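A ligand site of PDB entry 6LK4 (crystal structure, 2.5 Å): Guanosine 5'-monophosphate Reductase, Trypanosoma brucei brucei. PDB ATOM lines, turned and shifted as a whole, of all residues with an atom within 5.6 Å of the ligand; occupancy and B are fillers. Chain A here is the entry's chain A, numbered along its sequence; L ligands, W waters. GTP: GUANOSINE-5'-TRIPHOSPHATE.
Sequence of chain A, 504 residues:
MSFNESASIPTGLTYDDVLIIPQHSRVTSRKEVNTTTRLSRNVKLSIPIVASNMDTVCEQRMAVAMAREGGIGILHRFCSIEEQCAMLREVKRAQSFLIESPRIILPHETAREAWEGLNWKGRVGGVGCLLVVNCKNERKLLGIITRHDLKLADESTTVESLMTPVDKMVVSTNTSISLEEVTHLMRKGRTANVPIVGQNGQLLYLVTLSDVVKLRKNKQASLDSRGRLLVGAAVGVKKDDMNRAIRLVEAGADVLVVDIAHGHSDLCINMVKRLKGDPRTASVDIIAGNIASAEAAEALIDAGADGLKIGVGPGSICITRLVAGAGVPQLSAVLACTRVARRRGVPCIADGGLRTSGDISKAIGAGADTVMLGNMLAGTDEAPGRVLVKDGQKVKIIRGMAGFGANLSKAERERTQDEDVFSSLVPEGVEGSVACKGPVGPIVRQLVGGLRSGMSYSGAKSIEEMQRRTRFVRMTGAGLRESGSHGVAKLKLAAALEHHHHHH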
ATOM      1  N   ARG A  68       8.788  29.358   8.015  1.00  0.00           N
ATOM      2  CA  ARG A  68       7.401  29.393   7.568  1.00  0.00           C
ATOM      3  C   ARG A  68       6.678  30.602   8.104  1.00  0.00           C
ATOM      4  O   ARG A  68       5.804  31.156   7.428  1.00  0.00           O
ATOM      5  CB  ARG A  68       6.663  28.125   7.989  1.00  0.00           C
ATOM      6  CG  ARG A  68       7.053  26.917   7.192  1.00  0.00           C
ATOM      7  CD  ARG A  68       6.178  25.734   7.478  1.00  0.00           C
ATOM      8  NE  ARG A  68       6.456  24.688   6.501  1.00  0.00           N
ATOM      9  CZ  ARG A  68       6.430  23.380   6.763  1.00  0.00           C
ATOM     10  NH1 ARG A  68       6.118  22.961   7.983  1.00  0.00           N
ATOM     11  NH2 ARG A  68       6.708  22.505   5.800  1.00  0.00           N
ATOM     12  N   ARG A  93      14.957  20.003   3.012  1.00  0.00           N
ATOM     13  CA  ARG A  93      14.093  18.968   2.474  1.00  0.00           C
ATOM     14  C   ARG A  93      12.635  19.203   2.813  1.00  0.00           C
ATOM     15  O   ARG A  93      11.774  18.466   2.311  1.00  0.00           O
ATOM     16  CB  ARG A  93      14.558  17.608   3.005  1.00  0.00           C
ATOM     17  CG  ARG A  93      14.300  16.444   2.076  1.00  0.00           C
ATOM     18  CD  ARG A  93      15.030  16.582   0.766  1.00  0.00           C
ATOM     19  NE  ARG A  93      14.451  15.680  -0.206  1.00  0.00           N
ATOM     20  CZ  ARG A  93      15.116  14.720  -0.846  1.00  0.00           C
ATOM     21  NH1 ARG A  93      16.411  14.536  -0.643  1.00  0.00           N
ATOM     22  NH2 ARG A  93      14.480  13.931  -1.699  1.00  0.00           N
ATOM     23  N   ALA A  94      12.333  20.194   3.654  1.00  0.00           N
ATOM     24  CA  ALA A  94      10.981  20.314   4.189  1.00  0.00           C
ATOM     25  C   ALA A  94       9.969  20.685   3.099  1.00  0.00           C
ATOM     26  O   ALA A  94       8.873  20.115   3.040  1.00  0.00           O
ATOM     27  CB  ALA A  94      10.968  21.355   5.305  1.00  0.00           C
ATOM     28  N   GLN A  95      10.330  21.644   2.243  1.00  0.00           N
ATOM     29  CA  GLN A  95       9.540  21.955   1.069  1.00  0.00           C
ATOM     30  C   GLN A  95      10.465  22.448  -0.035  1.00  0.00           C
ATOM     31  O   GLN A  95      11.628  22.796   0.201  1.00  0.00           O
ATOM     32  CB  GLN A  95       8.464  22.987   1.381  1.00  0.00           C
ATOM     33  CG  GLN A  95       8.976  24.193   2.083  1.00  0.00           C
ATOM     34  CD  GLN A  95       7.929  25.280   2.154  1.00  0.00           C
ATOM     35  OE1 GLN A  95       7.182  25.361   3.136  1.00  0.00           O
ATOM     36  NE2 GLN A  95       7.860  26.123   1.130  1.00  0.00           N
ATOM     37  N   SER A  96       9.949  22.459  -1.257  1.00  0.00           N
ATOM     38  CA  SER A  96      10.726  22.957  -2.387  1.00  0.00           C
ATOM     39  C   SER A  96       9.758  23.200  -3.536  1.00  0.00           C
ATOM     40  O   SER A  96       8.564  22.911  -3.430  1.00  0.00           O
ATOM     41  CB  SER A  96      11.815  21.959  -2.803  1.00  0.00           C
ATOM     42  OG  SER A  96      12.529  22.443  -3.924  1.00  0.00           O
ATOM     43  N   ILE A  99      11.808  19.225  -6.414  1.00  0.00           N
ATOM     44  CA  ILE A  99      12.506  18.345  -5.497  1.00  0.00           C
ATOM     45  C   ILE A  99      13.659  17.708  -6.263  1.00  0.00           C
ATOM     46  O   ILE A  99      13.434  16.951  -7.204  1.00  0.00           O
ATOM     47  CB  ILE A  99      11.593  17.285  -4.896  1.00  0.00           C
ATOM     48  CG1 ILE A  99      10.387  17.947  -4.219  1.00  0.00           C
ATOM     49  CG2 ILE A  99      12.360  16.426  -3.902  1.00  0.00           C
ATOM     50  CD1 ILE A  99       9.206  17.028  -4.070  1.00  0.00           C
ATOM     51  N   SER A 101      16.512  14.949  -6.593  1.00  0.00           N
ATOM     52  CA  SER A 101      16.735  13.585  -6.106  1.00  0.00           C
ATOM     53  C   SER A 101      15.540  13.065  -5.311  1.00  0.00           C
ATOM     54  O   SER A 101      15.661  12.779  -4.108  1.00  0.00           O
ATOM     55  CB  SER A 101      18.005  13.550  -5.274  1.00  0.00           C
ATOM     56  N   PRO A 102      14.355  12.961  -5.912  1.00  0.00           N
ATOM     57  CA  PRO A 102      13.195  12.495  -5.148  1.00  0.00           C
ATOM     58  C   PRO A 102      13.309  11.021  -4.801  1.00  0.00           C
ATOM     59  O   PRO A 102      13.913  10.241  -5.539  1.00  0.00           O
ATOM     60  CB  PRO A 102      12.021  12.742  -6.101  1.00  0.00           C
ATOM     61  CG  PRO A 102      12.630  12.740  -7.465  1.00  0.00           C
ATOM     62  CD  PRO A 102      14.005  13.322  -7.297  1.00  0.00           C
ATOM     63  N   ARG A 103      12.721  10.657  -3.666  1.00  0.00           N
ATOM     64  CA  ARG A 103      12.836   9.269  -3.196  1.00  0.00           C
ATOM     65  C   ARG A 103      12.201   8.321  -4.203  1.00  0.00           C
ATOM     66  O   ARG A 103      11.102   8.565  -4.717  1.00  0.00           O
ATOM     67  CB  ARG A 103      12.180   9.101  -1.837  1.00  0.00           C
ATOM     68  CG  ARG A 103      12.710  10.060  -0.784  1.00  0.00           C
ATOM     69  CD  ARG A 103      14.220   9.975  -0.660  1.00  0.00           C
ATOM     70  NE  ARG A 103      14.618   8.783   0.087  1.00  0.00           N
ATOM     71  CZ  ARG A 103      15.866   8.399   0.293  1.00  0.00           C
ATOM     72  NH1 ARG A 103      16.885   9.099  -0.186  1.00  0.00           N
ATOM     73  NH2 ARG A 103      16.096   7.300   0.975  1.00  0.00           N
ATOM     74  N   TRP A 120      10.730   8.029   5.341  1.00  0.00           N
ATOM     75  CA  TRP A 120      12.146   8.361   5.293  1.00  0.00           C
ATOM     76  C   TRP A 120      12.484   9.345   6.405  1.00  0.00           C
ATOM     77  O   TRP A 120      11.714  10.258   6.711  1.00  0.00           O
ATOM     78  CB  TRP A 120      12.465   8.942   3.923  1.00  0.00           C
ATOM     79  CG  TRP A 120      13.891   9.290   3.664  1.00  0.00           C
ATOM     80  CD1 TRP A 120      14.978   8.500   3.847  1.00  0.00           C
ATOM     81  CD2 TRP A 120      14.377  10.524   3.083  1.00  0.00           C
ATOM     82  NE1 TRP A 120      16.121   9.159   3.448  1.00  0.00           N
ATOM     83  CE2 TRP A 120      15.773  10.402   2.977  1.00  0.00           C
ATOM     84  CE3 TRP A 120      13.759  11.704   2.653  1.00  0.00           C
ATOM     85  CZ2 TRP A 120      16.576  11.429   2.452  1.00  0.00           C
ATOM     86  CZ3 TRP A 120      14.561  12.727   2.145  1.00  0.00           C
ATOM     87  CH2 TRP A 120      15.950  12.574   2.042  1.00  0.00           C
ATOM     88  N   ARG A 123      13.318  13.624   5.992  1.00  0.00           N
ATOM     89  CA  ARG A 123      12.391  14.724   6.127  1.00  0.00           C
ATOM     90  C   ARG A 123      11.526  14.421   7.334  1.00  0.00           C
ATOM     91  O   ARG A 123      11.047  13.290   7.475  1.00  0.00           O
ATOM     92  CB  ARG A 123      11.523  14.888   4.878  1.00  0.00           C
ATOM     93  CG  ARG A 123      10.269  15.717   5.084  1.00  0.00           C
ATOM     94  CD  ARG A 123       9.665  16.045   3.742  1.00  0.00           C
ATOM     95  NE  ARG A 123       8.852  17.250   3.777  1.00  0.00           N
ATOM     96  CZ  ARG A 123       7.568  17.282   4.124  1.00  0.00           C
ATOM     97  NH1 ARG A 123       6.956  16.158   4.469  1.00  0.00           N
ATOM     98  NH2 ARG A 123       6.897  18.424   4.121  1.00  0.00           N
ATOM     99  N   GLY A 125       8.443  13.835   9.071  1.00  0.00           N
ATOM    100  CA  GLY A 125       7.171  13.432   8.535  1.00  0.00           C
ATOM    101  C   GLY A 125       7.271  12.517   7.341  1.00  0.00           C
ATOM    102  O   GLY A 125       6.238  12.050   6.854  1.00  0.00           O
ATOM    103  N   GLY A 126       8.488  12.237   6.858  1.00  0.00           N
ATOM    104  CA  GLY A 126       8.607  11.423   5.674  1.00  0.00           C
ATOM    105  C   GLY A 126       8.240  12.208   4.431  1.00  0.00           C
ATOM    106  O   GLY A 126       8.195  13.441   4.425  1.00  0.00           O
ATOM    107  N   VAL A 127       7.963  11.468   3.351  1.00  0.00           N
ATOM    108  CA  VAL A 127       7.645  12.042   2.059  1.00  0.00           C
ATOM    109  C   VAL A 127       6.282  11.517   1.608  1.00  0.00           C
ATOM    110  O   VAL A 127       5.801  10.486   2.080  1.00  0.00           O
ATOM    111  CB  VAL A 127       8.723  11.743   1.007  1.00  0.00           C
ATOM    112  CG1 VAL A 127      10.096  12.221   1.501  1.00  0.00           C
ATOM    113  CG2 VAL A 127       8.752  10.264   0.709  1.00  0.00           C
ATOM    114  N   GLY A 128       5.669  12.253   0.675  1.00  0.00           N
ATOM    115  CA  GLY A 128       4.310  11.967   0.262  1.00  0.00           C
ATOM    116  C   GLY A 128       4.158  10.909  -0.803  1.00  0.00           C
ATOM    117  O   GLY A 128       3.051  10.404  -1.008  1.00  0.00           O
ATOM    118  N   CYS A 129       5.228  10.543  -1.502  1.00  0.00           N
ATOM    119  CA  CYS A 129       5.086   9.484  -2.470  1.00  0.00           C
ATOM    120  C   CYS A 129       6.462   8.913  -2.741  1.00  0.00           C
ATOM    121  O   CYS A 129       7.477   9.509  -2.397  1.00  0.00           O
ATOM    122  CB  CYS A 129       4.438   9.972  -3.763  1.00  0.00           C
ATOM    123  SG  CYS A 129       5.630  10.751  -4.833  1.00  0.00           S
ATOM    124  N   LEU A 130       6.494   7.755  -3.358  1.00  0.00           N
ATOM    125  CA  LEU A 130       7.719   7.166  -3.859  1.00  0.00           C
ATOM    126  C   LEU A 130       7.556   6.984  -5.359  1.00  0.00           C
ATOM    127  O   LEU A 130       6.497   6.557  -5.838  1.00  0.00           O
ATOM    128  CB  LEU A 130       8.024   5.812  -3.217  1.00  0.00           C
ATOM    129  CG  LEU A 130       8.277   5.845  -1.710  1.00  0.00           C
ATOM    130  CD1 LEU A 130       8.393   4.425  -1.200  1.00  0.00           C
ATOM    131  CD2 LEU A 130       9.530   6.645  -1.391  1.00  0.00           C
ATOM    132  N   ARG A 147       0.883   6.372   0.221  1.00  0.00           N
ATOM    133  CA  ARG A 147       0.246   5.682   1.340  1.00  0.00           C
ATOM    134  C   ARG A 147      -1.137   5.178   0.946  1.00  0.00           C
ATOM    135  O   ARG A 147      -1.516   4.059   1.298  1.00  0.00           O
ATOM    136  CB  ARG A 147       0.132   6.599   2.551  1.00  0.00           C
ATOM    137  CG  ARG A 147       1.439   6.843   3.266  1.00  0.00           C
ATOM    138  CD  ARG A 147       1.335   8.043   4.221  1.00  0.00           C
ATOM    139  NE  ARG A 147       2.610   8.306   4.884  1.00  0.00           N
ATOM    140  CZ  ARG A 147       3.659   8.838   4.293  1.00  0.00           C
ATOM    141  NH1 ARG A 147       3.594   9.193   3.006  1.00  0.00           N
ATOM    142  NH2 ARG A 147       4.791   9.023   4.969  1.00  0.00           N
ATOM    143  N   ASN A 193       0.950  14.776  -7.997  1.00  0.00           N
ATOM    144  CA  ASN A 193       2.388  14.679  -8.195  1.00  0.00           C
ATOM    145  C   ASN A 193       2.678  14.713  -9.690  1.00  0.00           C
ATOM    146  O   ASN A 193       2.084  13.939 -10.451  1.00  0.00           O
ATOM    147  CB  ASN A 193       2.961  13.402  -7.590  1.00  0.00           C
ATOM    148  CG  ASN A 193       2.911  13.400  -6.075  1.00  0.00           C
ATOM    149  OD1 ASN A 193       3.749  14.018  -5.395  1.00  0.00           O
ATOM    150  ND2 ASN A 193       1.931  12.694  -5.534  1.00  0.00           N
ATOM    151  N   LEU A 206      10.676  16.160  -9.031  1.00  0.00           N
ATOM    152  CA  LEU A 206       9.289  15.941  -8.640  1.00  0.00           C
ATOM    153  C   LEU A 206       8.703  17.269  -8.197  1.00  0.00           C
ATOM    154  O   LEU A 206       9.345  18.013  -7.451  1.00  0.00           O
ATOM    155  CB  LEU A 206       9.172  14.899  -7.511  1.00  0.00           C
ATOM    156  CG  LEU A 206       7.733  14.711  -6.991  1.00  0.00           C
ATOM    157  CD1 LEU A 206       6.813  14.286  -8.144  1.00  0.00           C
ATOM    158  CD2 LEU A 206       7.623  13.728  -5.829  1.00  0.00           C
ATOM    159  N   THR A 208       5.172  18.534  -6.317  1.00  0.00           N
ATOM    160  CA  THR A 208       4.054  17.980  -5.571  1.00  0.00           C
ATOM    161  C   THR A 208       2.992  19.046  -5.393  1.00  0.00           C
ATOM    162  O   THR A 208       3.311  20.219  -5.216  1.00  0.00           O
ATOM    163  CB  THR A 208       4.450  17.444  -4.178  1.00  0.00           C
ATOM    164  OG1 THR A 208       4.630  18.533  -3.264  1.00  0.00           O
ATOM    165  CG2 THR A 208       5.726  16.635  -4.251  1.00  0.00           C
ATOM    166  N   SER A 210       1.345  19.413  -2.764  1.00  0.00           N
ATOM    167  CA  SER A 210       1.604  19.965  -1.435  1.00  0.00           C
ATOM    168  C   SER A 210       2.478  21.226  -1.503  1.00  0.00           C
ATOM    169  O   SER A 210       2.192  22.228  -0.850  1.00  0.00           O
ATOM    170  CB  SER A 210       2.239  18.887  -0.557  1.00  0.00           C
ATOM    171  OG  SER A 210       2.820  19.440   0.613  1.00  0.00           O
ATOM    172  N   ASP A 211       3.552  21.185  -2.304  1.00  0.00           N
ATOM    173  CA  ASP A 211       4.400  22.368  -2.419  1.00  0.00           C
ATOM    174  C   ASP A 211       3.700  23.497  -3.164  1.00  0.00           C
ATOM    175  O   ASP A 211       3.768  24.663  -2.757  1.00  0.00           O
ATOM    176  CB  ASP A 211       5.700  21.998  -3.108  1.00  0.00           C
ATOM    177  CG  ASP A 211       6.583  21.140  -2.233  1.00  0.00           C
ATOM    178  OD1 ASP A 211       6.822  21.524  -1.080  1.00  0.00           O
ATOM    179  OD2 ASP A 211       7.048  20.074  -2.704  1.00  0.00           O
ATOM    180  N   LYS A 214       1.552  25.402  -0.820  1.00  0.00           N
ATOM    181  CA  LYS A 214       2.300  26.282   0.073  1.00  0.00           C
ATOM    182  C   LYS A 214       2.779  27.526  -0.668  1.00  0.00           C
ATOM    183  O   LYS A 214       2.676  28.645  -0.146  1.00  0.00           O
ATOM    184  CB  LYS A 214       3.476  25.547   0.703  1.00  0.00           C
ATOM    185  CG  LYS A 214       3.127  24.685   1.873  1.00  0.00           C
ATOM    186  CD  LYS A 214       4.326  23.811   2.189  1.00  0.00           C
ATOM    187  CE  LYS A 214       3.939  22.530   2.894  1.00  0.00           C
ATOM    188  NZ  LYS A 214       4.912  21.405   2.607  1.00  0.00           N
HETATM  189  O3B GTP L   1       2.842  16.562   5.297  1.00  0.00           O
HETATM  190  PB  GTP L   1       2.849  17.313   3.873  1.00  0.00           P
HETATM  191  O1B GTP L   1       3.444  18.701   4.013  1.00  0.00           O
HETATM  192  O2B GTP L   1       1.432  17.388   3.313  1.00  0.00           O
HETATM  193  O3A GTP L   1       3.784  16.352   2.978  1.00  0.00           O
HETATM  194  PA  GTP L   1       3.250  15.312   1.868  1.00  0.00           P
HETATM  195  O1A GTP L   1       1.787  15.471   1.516  1.00  0.00           O
HETATM  196  O2A GTP L   1       3.573  13.928   2.343  1.00  0.00           O
HETATM  197  O5' GTP L   1       4.103  15.676   0.562  1.00  0.00           O
HETATM  198  C5' GTP L   1       5.506  15.530   0.552  1.00  0.00           C
HETATM  199  C4' GTP L   1       6.218  16.801   1.015  1.00  0.00           C
HETATM  200  O4' GTP L   1       7.529  16.407   1.363  1.00  0.00           O
HETATM  201  C3' GTP L   1       6.361  17.888  -0.028  1.00  0.00           C
HETATM  202  O3' GTP L   1       6.323  19.142   0.613  1.00  0.00           O
HETATM  203  C2' GTP L   1       7.757  17.667  -0.585  1.00  0.00           C
HETATM  204  O2' GTP L   1       8.394  18.833  -1.061  1.00  0.00           O
HETATM  205  C1' GTP L   1       8.498  17.088   0.599  1.00  0.00           C
HETATM  206  N9  GTP L   1       9.475  16.157   0.063  1.00  0.00           N
HETATM  207  C8  GTP L   1      10.825  16.223   0.246  1.00  0.00           C
HETATM  208  N7  GTP L   1      11.390  15.210  -0.442  1.00  0.00           N
HETATM  209  C5  GTP L   1      10.412  14.499  -1.052  1.00  0.00           C
HETATM  210  C6  GTP L   1      10.456  13.376  -1.862  1.00  0.00           C
HETATM  211  O6  GTP L   1      11.556  12.869  -2.109  1.00  0.00           O
HETATM  212  N1  GTP L   1       9.270  12.842  -2.351  1.00  0.00           N
HETATM  213  C2  GTP L   1       8.074  13.435  -2.038  1.00  0.00           C
HETATM  214  N2  GTP L   1       6.925  12.941  -2.502  1.00  0.00           N
HETATM  215  N3  GTP L   1       8.043  14.553  -1.228  1.00  0.00           N
HETATM  216  C4  GTP L   1       9.192  15.078  -0.744  1.00  0.00           C
HETATM  217  O   HOH W   1       4.367  13.805  -2.669  1.00  0.00           O
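OG1 of Thr 208 sits close to N of Ser 210 (3.4 Å). NH2 of Arg 123 sits at hydrogen-bond distance from O of Ala 94, at 2.8 Å. The backbone NH (N) of Ile 99 sits at hydrogen-bond distance from the backbone carbonyl oxygen (O) of Leu 206 (2.9 Å). NZ of Lys 214 sits at hydrogen-bond distance from OG of Ser 210, at 3.5 Å. OD2 of Asp 211 sits at hydrogen-bond distance from OG1 of Thr 208, 2.9 Å away. The guanidinium group (NE) of Arg 123 lies within hydrogen-bond range of the backbone carbonyl oxygen (O) of Arg 93. O of Ser 101 is in hydrogen-bond range of NH2 of Arg 93 (2.9 Å). The backbone carbonyl oxygen (O) of Val 127 sits at hydrogen-bond distance from the guanidinium group (NH1) of Arg 147.
O of Ala 94 touches O3' of the ligand (3.7 Å). CA of Gln 95 touches O2' of the ligand, 3.9 Å away. Ser 96 touches the ligand. Ile 99 touches the ligand. Pro 102 touches the ligand (CA to O6, 3.5 Å). Val 127 touches the ligand. Leu 206 touches the ligand (CD2 to N2, 3.5 Å). Thr 208 touches the ligand. Ser 210 touches the ligand. Of the 24 residues printed, 16 come within 4 Å of the ligand.
The side-chain carboxylate (OD2) of Asp 211 sits at hydrogen-bond distance from an oxygen (O2') of the ligand (2.5 Å). The guanidinium group of Arg 93 is in hydrogen-bond range of a nitrogen (N7) of the ligand (3.1 Å). The backbone carbonyl oxygen (O) of Cys 129 is in hydrogen-bond range of a nitrogen (N2) of the ligand (3.5 Å). An oxygen (O6) of the ligand lies within hydrogen-bond range of the backbone NH (N) of Arg 103 (2.9 Å). The side-chain amino group of Lys 214 lies within salt-bridge range of an oxygen (O1B) of the ligand (3.4 Å). N2 of the ligand is in hydrogen-bond range of SG of Cys 129. The guanidinium group of Arg 123 is in salt-bridge range of an oxygen (O1B) of the ligand (3.5 Å). The backbone NH (N) of Gly 128 sits close to an oxygen (O2A) of the ligand (3.2 Å).
Water W1 bridges a nitrogen (N2) of the ligand (2.7 Å) and the side-chain amide oxygen (OD1) of Asn 193 (2.8 Å).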
